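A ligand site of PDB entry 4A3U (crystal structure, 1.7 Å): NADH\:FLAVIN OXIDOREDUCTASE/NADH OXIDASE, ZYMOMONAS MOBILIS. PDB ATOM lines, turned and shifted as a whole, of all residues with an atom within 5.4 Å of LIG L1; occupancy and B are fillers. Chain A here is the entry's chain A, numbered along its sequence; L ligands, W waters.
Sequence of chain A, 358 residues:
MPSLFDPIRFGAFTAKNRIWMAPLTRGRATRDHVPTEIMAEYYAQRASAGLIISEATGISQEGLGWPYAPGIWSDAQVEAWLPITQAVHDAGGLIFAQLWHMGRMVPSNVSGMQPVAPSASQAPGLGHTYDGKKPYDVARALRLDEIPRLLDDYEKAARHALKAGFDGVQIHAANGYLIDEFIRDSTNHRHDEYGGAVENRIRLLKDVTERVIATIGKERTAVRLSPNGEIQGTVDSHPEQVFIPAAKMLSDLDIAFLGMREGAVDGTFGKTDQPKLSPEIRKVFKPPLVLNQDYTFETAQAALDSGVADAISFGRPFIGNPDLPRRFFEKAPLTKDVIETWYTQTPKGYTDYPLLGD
Water W2 lies within hydrogen-bond range of the backbone carbonyl oxygen (O) of Tyr 295 (2.8 Å) and an oxygen (O9) of LIG L1 (3.0 Å).
O2 of LIG L1 lies within hydrogen-bond range of OG1 of Thr 25 (2.6 Å).
N1 of LG2 L2 lies within hydrogen-bond range of OG1 of Thr 25, 3.0 Å away.
N of Ala 56 is in hydrogen-bond range of O2 of LIG L1, at 3.1 Å.
The guanidinium group of Arg 316 is in salt-bridge range of an oxygen (O8) of LIG L1, at 2.8 Å.
NE2 of His 172 lies within hydrogen-bond range of N2 of LG2 L2.
The side-chain amide oxygen of Gln 98 sits at hydrogen-bond distance from a nitrogen (N2) of LIG L1.
O1 of LIG L1 is in hydrogen-bond range of NE2 of His 172 (3.0 Å).
An oxygen (O1) of LG2 L2 lies within hydrogen-bond range of the side-chain amide nitrogen (ND2) of Asn 175, at 2.6 Å.
The backbone NH of Arg 316 is in hydrogen-bond range of an oxygen (O7) of LIG L1.
NH1 of Arg 224 lies within hydrogen-bond range of O1 of LIG L1.
An oxygen (O4) of LIG L1 lies within hydrogen-bond range of the side-chain amide oxygen (OD1) of Asn 292, at 2.6 Å.
N of Asp 294 is in hydrogen-bond range of O8 of LIG L1 (2.8 Å).
The backbone carbonyl oxygen (O) of Pro 23 lies close to an oxygen (O3) of LIG L1, 3.0 Å away.
N of Gly 315 lies within hydrogen-bond range of O9 of LIG L1, at 2.7 Å.
N3 of LIG L1 sits at hydrogen-bond distance from N of Thr 25, 2.7 Å away.
The guanidinium group (NH1) of Arg 316 lies within hydrogen-bond range of the backbone carbonyl oxygen (O) of Thr 268, 2.9 Å away.
ND2 of Asn 175 lies close to NH1 of Arg 224 (3.4 Å).
The guanidinium group (NE) of Arg 261 is in hydrogen-bond range of the side-chain amide oxygen (OD1) of Asn 175 (2.9 Å).
The side-chain carboxylate (OD1) of Asp 294 is in hydrogen-bond range of the side-chain hydroxyl (OG1) of Thr 268, at 2.6 Å.
The side-chain carboxylate (OD2) of Asp 294 sits at hydrogen-bond distance from the side-chain amide nitrogen (NE2) of Gln 293 (3.3 Å).
The side-chain amide nitrogen (ND2) of Asn 292 sits at hydrogen-bond distance from the backbone carbonyl oxygen (O) of Ser 313 (3.1 Å).
OE1 of Gln 293 is in hydrogen-bond range of NH1 of Arg 261 (2.7 Å).
The backbone NH (N) of Ala 22 is in hydrogen-bond range of the backbone carbonyl oxygen (O) of Phe 314, 3.0 Å away.
N1 of LIG L1 lies close to N2 of LG2 L2, at 3.3 Å.
Ala 22 touches LIG L1.
Leu 24 touches LIG L1.
ND2 of Asn 175 touches N1 of LIG L1 (3.5 Å).
Arg 261 touches LIG L1 (CD to O4, 3.3 Å).
CE2 of Phe 269 touches C9 of LIG L1, at 3.2 Å.
Gln 293 touches LIG L1 (CA to O6, 3.5 Å).
Phe 314 touches LIG L1.
CD of Pro 317 touches O7 of LIG L1 (3.9 Å).
Trp 342 touches LIG L1.
Tyr 343 touches LIG L1.
Hydrophobic or aromatic side chains within 4 Å of LIG L1: Ala 22, Pro 23, Leu 24, Ala 56, His 172, Phe 269, Pro 317, Trp 342 and Tyr 343.
Within 4 Å of LIG L1: Ala 22, Pro 23, Leu 24, Thr 25, Ala 56, Gln 98, His 172, Asn 175, Arg 224, Arg 261, Phe 269, Asn 292, Gln 293, Asp 294, Phe 314, Gly 315, Arg 316, Pro 317, Trp 342 and Tyr 343.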
ATOM      1  N   ALA A  22      22.365  22.864  12.349  1.00  0.00           N
ATOM      2  CA  ALA A  22      22.204  23.625  13.578  1.00  0.00           C
ATOM      3  C   ALA A  22      21.834  22.662  14.683  1.00  0.00           C
ATOM      4  O   ALA A  22      21.155  21.657  14.398  1.00  0.00           O
ATOM      5  CB  ALA A  22      21.087  24.668  13.392  1.00  0.00           C
ATOM      6  N   PRO A  23      22.250  22.953  15.919  1.00  0.00           N
ATOM      7  CA  PRO A  23      21.794  22.219  17.102  1.00  0.00           C
ATOM      8  C   PRO A  23      20.275  22.115  17.238  1.00  0.00           C
ATOM      9  O   PRO A  23      19.565  23.134  17.269  1.00  0.00           O
ATOM     10  CB  PRO A  23      22.365  23.013  18.276  1.00  0.00           C
ATOM     11  CG  PRO A  23      22.643  24.398  17.705  1.00  0.00           C
ATOM     12  CD  PRO A  23      22.896  24.248  16.264  1.00  0.00           C
ATOM     13  N   LEU A  24      19.785  20.880  17.337  1.00  0.00           N
ATOM     14  CA  LEU A  24      18.339  20.579  17.388  1.00  0.00           C
ATOM     15  C   LEU A  24      17.969  19.616  18.535  1.00  0.00           C
ATOM     16  O   LEU A  24      18.335  18.444  18.456  1.00  0.00           O
ATOM     17  CB  LEU A  24      17.927  19.992  16.046  1.00  0.00           C
ATOM     18  CG  LEU A  24      17.916  21.035  14.887  1.00  0.00           C
ATOM     19  CD1 LEU A  24      18.128  20.359  13.524  1.00  0.00           C
ATOM     20  CD2 LEU A  24      16.705  21.972  14.850  1.00  0.00           C
ATOM     21  N   THR A  25      17.309  20.117  19.605  1.00  0.00           N
ATOM     22  CA  THR A  25      16.865  19.293  20.761  1.00  0.00           C
ATOM     23  C   THR A  25      15.714  18.447  20.230  1.00  0.00           C
ATOM     24  O   THR A  25      14.771  18.995  19.709  1.00  0.00           O
ATOM     25  CB  THR A  25      16.428  20.152  21.944  1.00  0.00           C
ATOM     26  OG1 THR A  25      17.592  20.710  22.534  1.00  0.00           O
ATOM     27  CG2 THR A  25      15.664  19.347  23.085  1.00  0.00           C
ATOM     28  N   ARG A  26      15.816  17.144  20.433  1.00  0.00           N
ATOM     29  CA  ARG A  26      14.819  16.179  19.907  1.00  0.00           C
ATOM     30  C   ARG A  26      14.196  15.265  20.946  1.00  0.00           C
ATOM     31  O   ARG A  26      13.149  14.684  20.669  1.00  0.00           O
ATOM     32  CB  ARG A  26      15.437  15.340  18.767  1.00  0.00           C
ATOM     33  CG  ARG A  26      16.028  16.145  17.602  1.00  0.00           C
ATOM     34  CD  ARG A  26      15.145  17.218  16.976  1.00  0.00           C
ATOM     35  NE  ARG A  26      13.859  16.735  16.517  1.00  0.00           N
ATOM     36  CZ  ARG A  26      13.606  16.087  15.378  1.00  0.00           C
ATOM     37  NH1 ARG A  26      14.579  15.794  14.507  1.00  0.00           N
ATOM     38  NH2 ARG A  26      12.349  15.658  15.153  1.00  0.00           N
ATOM     39  N   SER A  54      25.456  18.945  17.482  1.00  0.00           N
ATOM     40  CA  SER A  54      24.519  18.091  18.175  1.00  0.00           C
ATOM     41  C   SER A  54      23.364  18.881  18.794  1.00  0.00           C
ATOM     42  O   SER A  54      23.443  20.076  19.101  1.00  0.00           O
ATOM     43  CB  SER A  54      25.199  17.285  19.303  1.00  0.00           C
ATOM     44  OG  SER A  54      25.337  17.933  20.553  1.00  0.00           O
ATOM     45  N   GLU A  55      22.280  18.161  19.051  1.00  0.00           N
ATOM     46  CA  GLU A  55      21.312  18.627  20.024  1.00  0.00           C
ATOM     47  C   GLU A  55      21.997  19.048  21.317  1.00  0.00           C
ATOM     48  O   GLU A  55      23.042  18.519  21.681  1.00  0.00           O
ATOM     49  CB  GLU A  55      20.377  17.455  20.398  1.00  0.00           C
ATOM     50  CG  GLU A  55      21.034  16.355  21.178  1.00  0.00           C
ATOM     51  CD  GLU A  55      20.412  15.011  20.854  1.00  0.00           C
ATOM     52  OE1 GLU A  55      20.603  14.421  19.764  1.00  0.00           O
ATOM     53  OE2 GLU A  55      19.662  14.583  21.684  1.00  0.00           O
ATOM     54  N   ALA A  56      21.354  19.937  22.045  1.00  0.00           N
ATOM     55  CA  ALA A  56      21.913  20.480  23.278  1.00  0.00           C
ATOM     56  C   ALA A  56      22.120  19.364  24.259  1.00  0.00           C
ATOM     57  O   ALA A  56      21.205  18.588  24.474  1.00  0.00           O
ATOM     58  CB  ALA A  56      20.996  21.558  23.846  1.00  0.00           C
ATOM     59  N   GLN A  98      27.055  20.088  21.483  1.00  0.00           N
ATOM     60  CA  GLN A  98      26.639  21.341  22.148  1.00  0.00           C
ATOM     61  C   GLN A  98      26.547  21.135  23.655  1.00  0.00           C
ATOM     62  O   GLN A  98      25.821  20.316  24.138  1.00  0.00           O
ATOM     63  CB  GLN A  98      25.292  21.866  21.602  1.00  0.00           C
ATOM     64  CG  GLN A  98      25.215  23.378  21.685  1.00  0.00           C
ATOM     65  CD  GLN A  98      23.837  23.959  21.383  1.00  0.00           C
ATOM     66  OE1 GLN A  98      22.781  23.339  21.623  1.00  0.00           O
ATOM     67  NE2 GLN A  98      23.851  25.165  20.804  1.00  0.00           N
ATOM     68  N   TRP A 100      25.636  22.214  27.376  1.00  0.00           N
ATOM     69  CA  TRP A 100      24.358  22.855  27.764  1.00  0.00           C
ATOM     70  C   TRP A 100      24.220  22.970  29.231  1.00  0.00           C
ATOM     71  O   TRP A 100      24.318  21.943  29.975  1.00  0.00           O
ATOM     72  CB  TRP A 100      23.134  22.052  27.244  1.00  0.00           C
ATOM     73  CG  TRP A 100      21.870  22.845  26.947  1.00  0.00           C
ATOM     74  CD1 TRP A 100      21.764  24.197  26.696  1.00  0.00           C
ATOM     75  CD2 TRP A 100      20.507  22.293  26.707  1.00  0.00           C
ATOM     76  NE1 TRP A 100      20.470  24.539  26.430  1.00  0.00           N
ATOM     77  CE2 TRP A 100      19.678  23.441  26.401  1.00  0.00           C
ATOM     78  CE3 TRP A 100      19.931  21.017  26.764  1.00  0.00           C
ATOM     79  CZ2 TRP A 100      18.316  23.309  26.119  1.00  0.00           C
ATOM     80  CZ3 TRP A 100      18.580  20.890  26.453  1.00  0.00           C
ATOM     81  CH2 TRP A 100      17.781  21.996  26.168  1.00  0.00           C
ATOM     82  N   HIS A 172      26.971  26.293  24.571  1.00  0.00           N
ATOM     83  CA  HIS A 172      25.661  26.939  24.428  1.00  0.00           C
ATOM     84  C   HIS A 172      25.629  28.193  25.271  1.00  0.00           C
ATOM     85  O   HIS A 172      25.524  28.123  26.512  1.00  0.00           O
ATOM     86  CB  HIS A 172      24.534  25.988  24.808  1.00  0.00           C
ATOM     87  CG  HIS A 172      23.226  26.361  24.176  1.00  0.00           C
ATOM     88  ND1 HIS A 172      22.890  27.641  23.858  1.00  0.00           N
ATOM     89  CD2 HIS A 172      22.166  25.576  23.799  1.00  0.00           C
ATOM     90  CE1 HIS A 172      21.688  27.634  23.314  1.00  0.00           C
ATOM     91  NE2 HIS A 172      21.248  26.391  23.301  1.00  0.00           N
ATOM     92  N   ASN A 175      20.025  31.870  23.566  1.00  0.00           N
ATOM     93  CA  ASN A 175      18.648  31.422  23.609  1.00  0.00           C
ATOM     94  C   ASN A 175      18.075  31.497  24.996  1.00  0.00           C
ATOM     95  O   ASN A 175      17.074  30.891  25.286  1.00  0.00           O
ATOM     96  CB  ASN A 175      18.470  30.062  22.902  1.00  0.00           C
ATOM     97  CG  ASN A 175      18.829  30.152  21.390  1.00  0.00           C
ATOM     98  OD1 ASN A 175      19.081  31.201  20.867  1.00  0.00           O
ATOM     99  ND2 ASN A 175      18.907  29.011  20.716  1.00  0.00           N
ATOM    100  N   ARG A 224      28.157  29.309  20.690  1.00  0.00           N
ATOM    101  CA  ARG A 224      26.939  29.897  20.212  1.00  0.00           C
ATOM    102  C   ARG A 224      26.462  31.094  21.016  1.00  0.00           C
ATOM    103  O   ARG A 224      26.315  31.002  22.231  1.00  0.00           O
ATOM    104  CB  ARG A 224      25.785  28.878  20.144  1.00  0.00           C
ATOM    105  CG  ARG A 224      24.893  29.158  18.927  1.00  0.00           C
ATOM    106  CD  ARG A 224      23.749  28.146  18.881  1.00  0.00           C
ATOM    107  NE  ARG A 224      23.177  27.995  17.555  1.00  0.00           N
ATOM    108  CZ  ARG A 224      21.888  27.772  17.289  1.00  0.00           C
ATOM    109  NH1 ARG A 224      20.938  27.759  18.233  1.00  0.00           N
ATOM    110  NH2 ARG A 224      21.523  27.614  16.025  1.00  0.00           N
ATOM    111  N   ARG A 261      22.504  32.450  16.034  1.00  0.00           N
ATOM    112  CA  ARG A 261      21.135  32.486  15.534  1.00  0.00           C
ATOM    113  C   ARG A 261      20.654  33.927  15.578  1.00  0.00           C
ATOM    114  O   ARG A 261      20.647  34.534  16.650  1.00  0.00           O
ATOM    115  CB  ARG A 261      20.242  31.653  16.469  1.00  0.00           C
ATOM    116  CG  ARG A 261      18.759  31.701  16.110  1.00  0.00           C
ATOM    117  CD  ARG A 261      17.790  31.102  17.135  1.00  0.00           C
ATOM    118  NE  ARG A 261      17.741  31.853  18.376  1.00  0.00           N
ATOM    119  CZ  ARG A 261      17.253  33.088  18.557  1.00  0.00           C
ATOM    120  NH1 ARG A 261      16.602  33.738  17.588  1.00  0.00           N
ATOM    121  NH2 ARG A 261      17.330  33.634  19.756  1.00  0.00           N
ATOM    122  N   THR A 268      10.885  33.494  12.182  1.00  0.00           N
ATOM    123  CA  THR A 268      10.047  32.320  12.462  1.00  0.00           C
ATOM    124  C   THR A 268      10.645  31.387  13.518  1.00  0.00           C
ATOM    125  O   THR A 268      10.007  30.408  13.895  1.00  0.00           O
ATOM    126  CB  THR A 268       9.590  31.561  11.164  1.00  0.00           C
ATOM    127  OG1 THR A 268      10.618  30.709  10.651  1.00  0.00           O
ATOM    128  CG2 THR A 268       9.173  32.559  10.074  1.00  0.00           C
ATOM    129  N   PHE A 269      11.821  31.715  14.037  1.00  0.00           N
ATOM    130  CA  PHE A 269      12.284  31.158  15.327  1.00  0.00           C
ATOM    131  C   PHE A 269      12.919  32.240  16.209  1.00  0.00           C
ATOM    132  O   PHE A 269      13.958  32.020  16.842  1.00  0.00           O
ATOM    133  CB  PHE A 269      13.238  29.955  15.141  1.00  0.00           C
ATOM    134  CG  PHE A 269      13.087  28.929  16.226  1.00  0.00           C
ATOM    135  CD1 PHE A 269      13.833  29.007  17.410  1.00  0.00           C
ATOM    136  CD2 PHE A 269      12.166  27.885  16.083  1.00  0.00           C
ATOM    137  CE1 PHE A 269      13.704  28.060  18.417  1.00  0.00           C
ATOM    138  CE2 PHE A 269      12.005  26.946  17.093  1.00  0.00           C
ATOM    139  CZ  PHE A 269      12.777  27.020  18.262  1.00  0.00           C
ATOM    140  N   ASN A 292      22.715  31.769  11.273  1.00  0.00           N
ATOM    141  CA  ASN A 292      21.551  30.875  11.341  1.00  0.00           C
ATOM    142  C   ASN A 292      20.241  31.651  11.531  1.00  0.00           C
ATOM    143  O   ASN A 292      20.213  32.749  12.055  1.00  0.00           O
ATOM    144  CB  ASN A 292      21.734  29.855  12.449  1.00  0.00           C
ATOM    145  CG  ASN A 292      20.480  29.134  12.796  1.00  0.00           C
ATOM    146  OD1 ASN A 292      19.802  29.530  13.743  1.00  0.00           O
ATOM    147  ND2 ASN A 292      20.108  28.115  11.977  1.00  0.00           N
ATOM    148  N   GLN A 293      19.167  30.934  11.183  1.00  0.00           N
ATOM    149  CA  GLN A 293      17.753  31.259  11.450  1.00  0.00           C
ATOM    150  C   GLN A 293      17.186  31.808  10.171  1.00  0.00           C
ATOM    151  O   GLN A 293      17.640  32.864   9.718  1.00  0.00           O
ATOM    152  CB  GLN A 293      17.472  32.233  12.628  1.00  0.00           C
ATOM    153  CG  GLN A 293      15.958  32.314  12.896  1.00  0.00           C
ATOM    154  CD  GLN A 293      15.571  33.316  13.906  1.00  0.00           C
ATOM    155  OE1 GLN A 293      16.068  33.254  15.028  1.00  0.00           O
ATOM    156  NE2 GLN A 293      14.582  34.222  13.557  1.00  0.00           N
ATOM    157  N   ASP A 294      16.247  31.055   9.598  1.00  0.00           N
ATOM    158  CA  ASP A 294      15.353  31.488   8.465  1.00  0.00           C
ATOM    159  C   ASP A 294      16.034  31.557   7.050  1.00  0.00           C
ATOM    160  O   ASP A 294      15.482  32.182   6.145  1.00  0.00           O
ATOM    161  CB  ASP A 294      14.704  32.846   8.763  1.00  0.00           C
ATOM    162  CG  ASP A 294      13.516  32.744   9.764  1.00  0.00           C
ATOM    163  OD1 ASP A 294      12.755  31.755   9.687  1.00  0.00           O
ATOM    164  OD2 ASP A 294      13.342  33.663  10.601  1.00  0.00           O
ATOM    165  N   TYR A 295      17.207  30.970   6.902  1.00  0.00           N
ATOM    166  CA  TYR A 295      17.945  31.064   5.639  1.00  0.00           C
ATOM    167  C   TYR A 295      17.292  30.098   4.687  1.00  0.00           C
ATOM    168  O   TYR A 295      17.006  28.951   5.072  1.00  0.00           O
ATOM    169  CB  TYR A 295      19.456  30.752   5.749  1.00  0.00           C
ATOM    170  CG  TYR A 295      20.268  31.946   6.273  1.00  0.00           C
ATOM    171  CD1 TYR A 295      20.415  32.145   7.632  1.00  0.00           C
ATOM    172  CD2 TYR A 295      20.796  32.896   5.395  1.00  0.00           C
ATOM    173  CE1 TYR A 295      21.136  33.242   8.139  1.00  0.00           C
ATOM    174  CE2 TYR A 295      21.498  34.005   5.867  1.00  0.00           C
ATOM    175  CZ  TYR A 295      21.659  34.184   7.262  1.00  0.00           C
ATOM    176  OH  TYR A 295      22.387  35.300   7.789  1.00  0.00           O
ATOM    177  N   SER A 313      24.185  27.453   9.124  1.00  0.00           N
ATOM    178  CA  SER A 313      23.543  26.231   9.633  1.00  0.00           C
ATOM    179  C   SER A 313      22.077  26.233   9.325  1.00  0.00           C
ATOM    180  O   SER A 313      21.445  27.274   9.296  1.00  0.00           O
ATOM    181  CB  SER A 313      23.745  26.069  11.131  1.00  0.00           C
ATOM    182  OG  SER A 313      23.369  27.181  11.904  1.00  0.00           O
ATOM    183  N   PHE A 314      21.515  25.041   9.168  1.00  0.00           N
ATOM    184  CA  PHE A 314      20.088  24.937   8.880  1.00  0.00           C
ATOM    185  C   PHE A 314      19.525  24.115   9.992  1.00  0.00           C
ATOM    186  O   PHE A 314      20.113  23.091  10.358  1.00  0.00           O
ATOM    187  CB  PHE A 314      19.872  24.289   7.522  1.00  0.00           C
ATOM    188  CG  PHE A 314      20.312  25.185   6.408  1.00  0.00           C
ATOM    189  CD1 PHE A 314      21.660  25.299   6.125  1.00  0.00           C
ATOM    190  CD2 PHE A 314      19.416  25.974   5.723  1.00  0.00           C
ATOM    191  CE1 PHE A 314      22.084  26.136   5.118  1.00  0.00           C
ATOM    192  CE2 PHE A 314      19.827  26.831   4.721  1.00  0.00           C
ATOM    193  CZ  PHE A 314      21.155  26.922   4.416  1.00  0.00           C
ATOM    194  N   GLY A 315      18.386  24.578  10.531  1.00  0.00           N
ATOM    195  CA  GLY A 315      17.720  23.877  11.587  1.00  0.00           C
ATOM    196  C   GLY A 315      16.547  23.044  11.122  1.00  0.00           C
ATOM    197  O   GLY A 315      16.676  21.875  10.862  1.00  0.00           O
ATOM    198  N   ARG A 316      15.381  23.660  11.041  1.00  0.00           N
ATOM    199  CA  ARG A 316      14.200  22.880  10.722  1.00  0.00           C
ATOM    200  C   ARG A 316      14.347  22.174   9.361  1.00  0.00           C
ATOM    201  O   ARG A 316      13.915  21.043   9.212  1.00  0.00           O
ATOM    202  CB  ARG A 316      12.973  23.757  10.833  1.00  0.00           C
ATOM    203  CG  ARG A 316      12.742  24.222  12.280  1.00  0.00           C
ATOM    204  CD  ARG A 316      11.860  25.440  12.324  1.00  0.00           C
ATOM    205  NE  ARG A 316      12.632  26.666  12.096  1.00  0.00           N
ATOM    206  CZ  ARG A 316      12.132  27.896  12.132  1.00  0.00           C
ATOM    207  NH1 ARG A 316      10.836  28.067  12.420  1.00  0.00           N
ATOM    208  NH2 ARG A 316      12.926  28.957  11.898  1.00  0.00           N
ATOM    209  N   PRO A 317      14.994  22.805   8.351  1.00  0.00           N
ATOM    210  CA  PRO A 317      15.214  22.055   7.102  1.00  0.00           C
ATOM    211  C   PRO A 317      15.881  20.712   7.258  1.00  0.00           C
ATOM    212  O   PRO A 317      15.464  19.803   6.540  1.00  0.00           O
ATOM    213  CB  PRO A 317      16.093  22.990   6.275  1.00  0.00           C
ATOM    214  CG  PRO A 317      15.557  24.326   6.680  1.00  0.00           C
ATOM    215  CD  PRO A 317      15.372  24.213   8.167  1.00  0.00           C
ATOM    216  N   ILE A 319      15.627  18.690   9.720  1.00  0.00           N
ATOM    217  CA  ILE A 319      14.710  17.859  10.434  1.00  0.00           C
ATOM    218  C   ILE A 319      13.974  16.967   9.425  1.00  0.00           C
ATOM    219  O   ILE A 319      13.908  15.755   9.605  1.00  0.00           O
ATOM    220  CB  ILE A 319      13.694  18.635  11.308  1.00  0.00           C
ATOM    221  CG1 ILE A 319      14.328  19.216  12.571  1.00  0.00           C
ATOM    222  CG2 ILE A 319      12.576  17.691  11.761  1.00  0.00           C
ATOM    223  CD1 ILE A 319      13.377  20.105  13.372  1.00  0.00           C
ATOM    224  N   TRP A 342       8.675  17.286  16.836  1.00  0.00           N
ATOM    225  CA  TRP A 342       9.999  17.874  17.166  1.00  0.00           C
ATOM    226  C   TRP A 342      10.605  17.277  18.376  1.00  0.00           C
ATOM    227  O   TRP A 342      11.837  16.936  18.384  1.00  0.00           O
ATOM    228  CB  TRP A 342       9.823  19.342  17.430  1.00  0.00           C
ATOM    229  CG  TRP A 342       9.754  20.244  16.216  1.00  0.00           C
ATOM    230  CD1 TRP A 342      10.007  19.942  14.876  1.00  0.00           C
ATOM    231  CD2 TRP A 342       9.502  21.662  16.245  1.00  0.00           C
ATOM    232  NE1 TRP A 342       9.892  21.097  14.083  1.00  0.00           N
ATOM    233  CE2 TRP A 342       9.590  22.152  14.856  1.00  0.00           C
ATOM    234  CE3 TRP A 342       9.268  22.584  17.265  1.00  0.00           C
ATOM    235  CZ2 TRP A 342       9.431  23.489  14.545  1.00  0.00           C
ATOM    236  CZ3 TRP A 342       9.066  23.912  16.915  1.00  0.00           C
ATOM    237  CH2 TRP A 342       9.158  24.352  15.574  1.00  0.00           C
ATOM    238  N   TYR A 343       9.753  17.134  19.418  1.00  0.00           N
ATOM    239  CA  TYR A 343      10.131  16.735  20.754  1.00  0.00           C
ATOM    240  C   TYR A 343       9.350  15.575  21.341  1.00  0.00           C
ATOM    241  O   TYR A 343       9.415  15.366  22.530  1.00  0.00           O
ATOM    242  CB  TYR A 343       9.942  17.875  21.744  1.00  0.00           C
ATOM    243  CG  TYR A 343      10.439  19.244  21.301  1.00  0.00           C
ATOM    244  CD1 TYR A 343      11.781  19.515  21.172  1.00  0.00           C
ATOM    245  CD2 TYR A 343       9.551  20.300  21.097  1.00  0.00           C
ATOM    246  CE1 TYR A 343      12.231  20.772  20.826  1.00  0.00           C
ATOM    247  CE2 TYR A 343      10.000  21.570  20.739  1.00  0.00           C
ATOM    248  CZ  TYR A 343      11.340  21.806  20.583  1.00  0.00           C
ATOM    249  OH  TYR A 343      11.776  23.073  20.222  1.00  0.00           O
HETATM  250  N1  LIG L   1      19.269  25.727  19.422  1.00  0.00           N
HETATM  251  C1  LIG L   1      20.224  25.348  20.232  1.00  0.00           C
HETATM  252  O1  LIG L   1      21.111  26.225  20.348  1.00  0.00           O
HETATM  253  N2  LIG L   1      20.270  24.128  20.866  1.00  0.00           N
HETATM  254  C2  LIG L   1      19.253  23.248  20.694  1.00  0.00           C
HETATM  255  O2  LIG L   1      19.355  22.135  21.275  1.00  0.00           O
HETATM  256  C3  LIG L   1      18.134  23.621  19.771  1.00  0.00           C
HETATM  257  N3  LIG L   1      17.080  22.810  19.532  1.00  0.00           N
HETATM  258  C4  LIG L   1      16.065  23.132  18.686  1.00  0.00           C
HETATM  259  C5  LIG L   1      15.016  22.212  18.451  1.00  0.00           C
HETATM  260  C6  LIG L   1      13.995  22.503  17.557  1.00  0.00           C
HETATM  261  C7  LIG L   1      12.914  21.497  17.337  1.00  0.00           C
HETATM  262  C8  LIG L   1      13.972  23.801  16.877  1.00  0.00           C
HETATM  263  C9  LIG L   1      12.864  24.132  15.950  1.00  0.00           C
HETATM  264  C10 LIG L   1      14.991  24.727  17.105  1.00  0.00           C
HETATM  265  C11 LIG L   1      16.068  24.450  17.957  1.00  0.00           C
HETATM  266  N4  LIG L   1      17.161  25.354  18.213  1.00  0.00           N
HETATM  267  C12 LIG L   1      18.190  24.954  19.101  1.00  0.00           C
HETATM  268  C13 LIG L   1      17.111  26.622  17.479  1.00  0.00           C
HETATM  269  C14 LIG L   1      17.632  26.145  16.091  1.00  0.00           C
HETATM  270  O3  LIG L   1      19.006  25.846  16.111  1.00  0.00           O
HETATM  271  C15 LIG L   1      17.632  27.158  14.999  1.00  0.00           C
HETATM  272  O4  LIG L   1      18.419  28.227  15.554  1.00  0.00           O
HETATM  273  C16 LIG L   1      16.245  27.451  14.526  1.00  0.00           C
HETATM  274  O5  LIG L   1      15.729  26.193  14.007  1.00  0.00           O
HETATM  275  C17 LIG L   1      16.311  28.553  13.477  1.00  0.00           C
HETATM  276  O6  LIG L   1      16.947  27.995  12.326  1.00  0.00           O
HETATM  277  P1  LIG L   1      16.249  27.488  11.021  1.00  0.00           P
HETATM  278  O7  LIG L   1      15.456  26.253  11.440  1.00  0.00           O
HETATM  279  O8  LIG L   1      15.354  28.629  10.589  1.00  0.00           O
HETATM  280  O9  LIG L   1      17.371  27.045  10.105  1.00  0.00           O
HETATM  281  N1  LG2 L   2      16.107  23.269  22.846  1.00  0.00           N
HETATM  282  C1  LG2 L   2      16.909  24.325  22.748  1.00  0.00           C
HETATM  283  C2  LG2 L   2      16.436  25.524  22.177  1.00  0.00           C
HETATM  284  C3  LG2 L   2      15.135  25.624  21.703  1.00  0.00           C
HETATM  285  C4  LG2 L   2      14.310  24.500  21.825  1.00  0.00           C
HETATM  286  C5  LG2 L   2      14.823  23.347  22.399  1.00  0.00           C
HETATM  287  C6  LG2 L   2      17.299  26.766  22.047  1.00  0.00           C
HETATM  288  O1  LG2 L   2      16.769  27.766  21.551  1.00  0.00           O
HETATM  289  N2  LG2 L   2      18.538  26.739  22.510  1.00  0.00           N
HETATM  290  O   HOH W   1      13.785  27.910   8.173  1.00  0.00           O
HETATM  291  O   HOH W   2      16.425  27.268   7.284  1.00  0.00           O
HETATM  292  O   HOH W   3      18.940  28.930   9.264  1.00  0.00           O
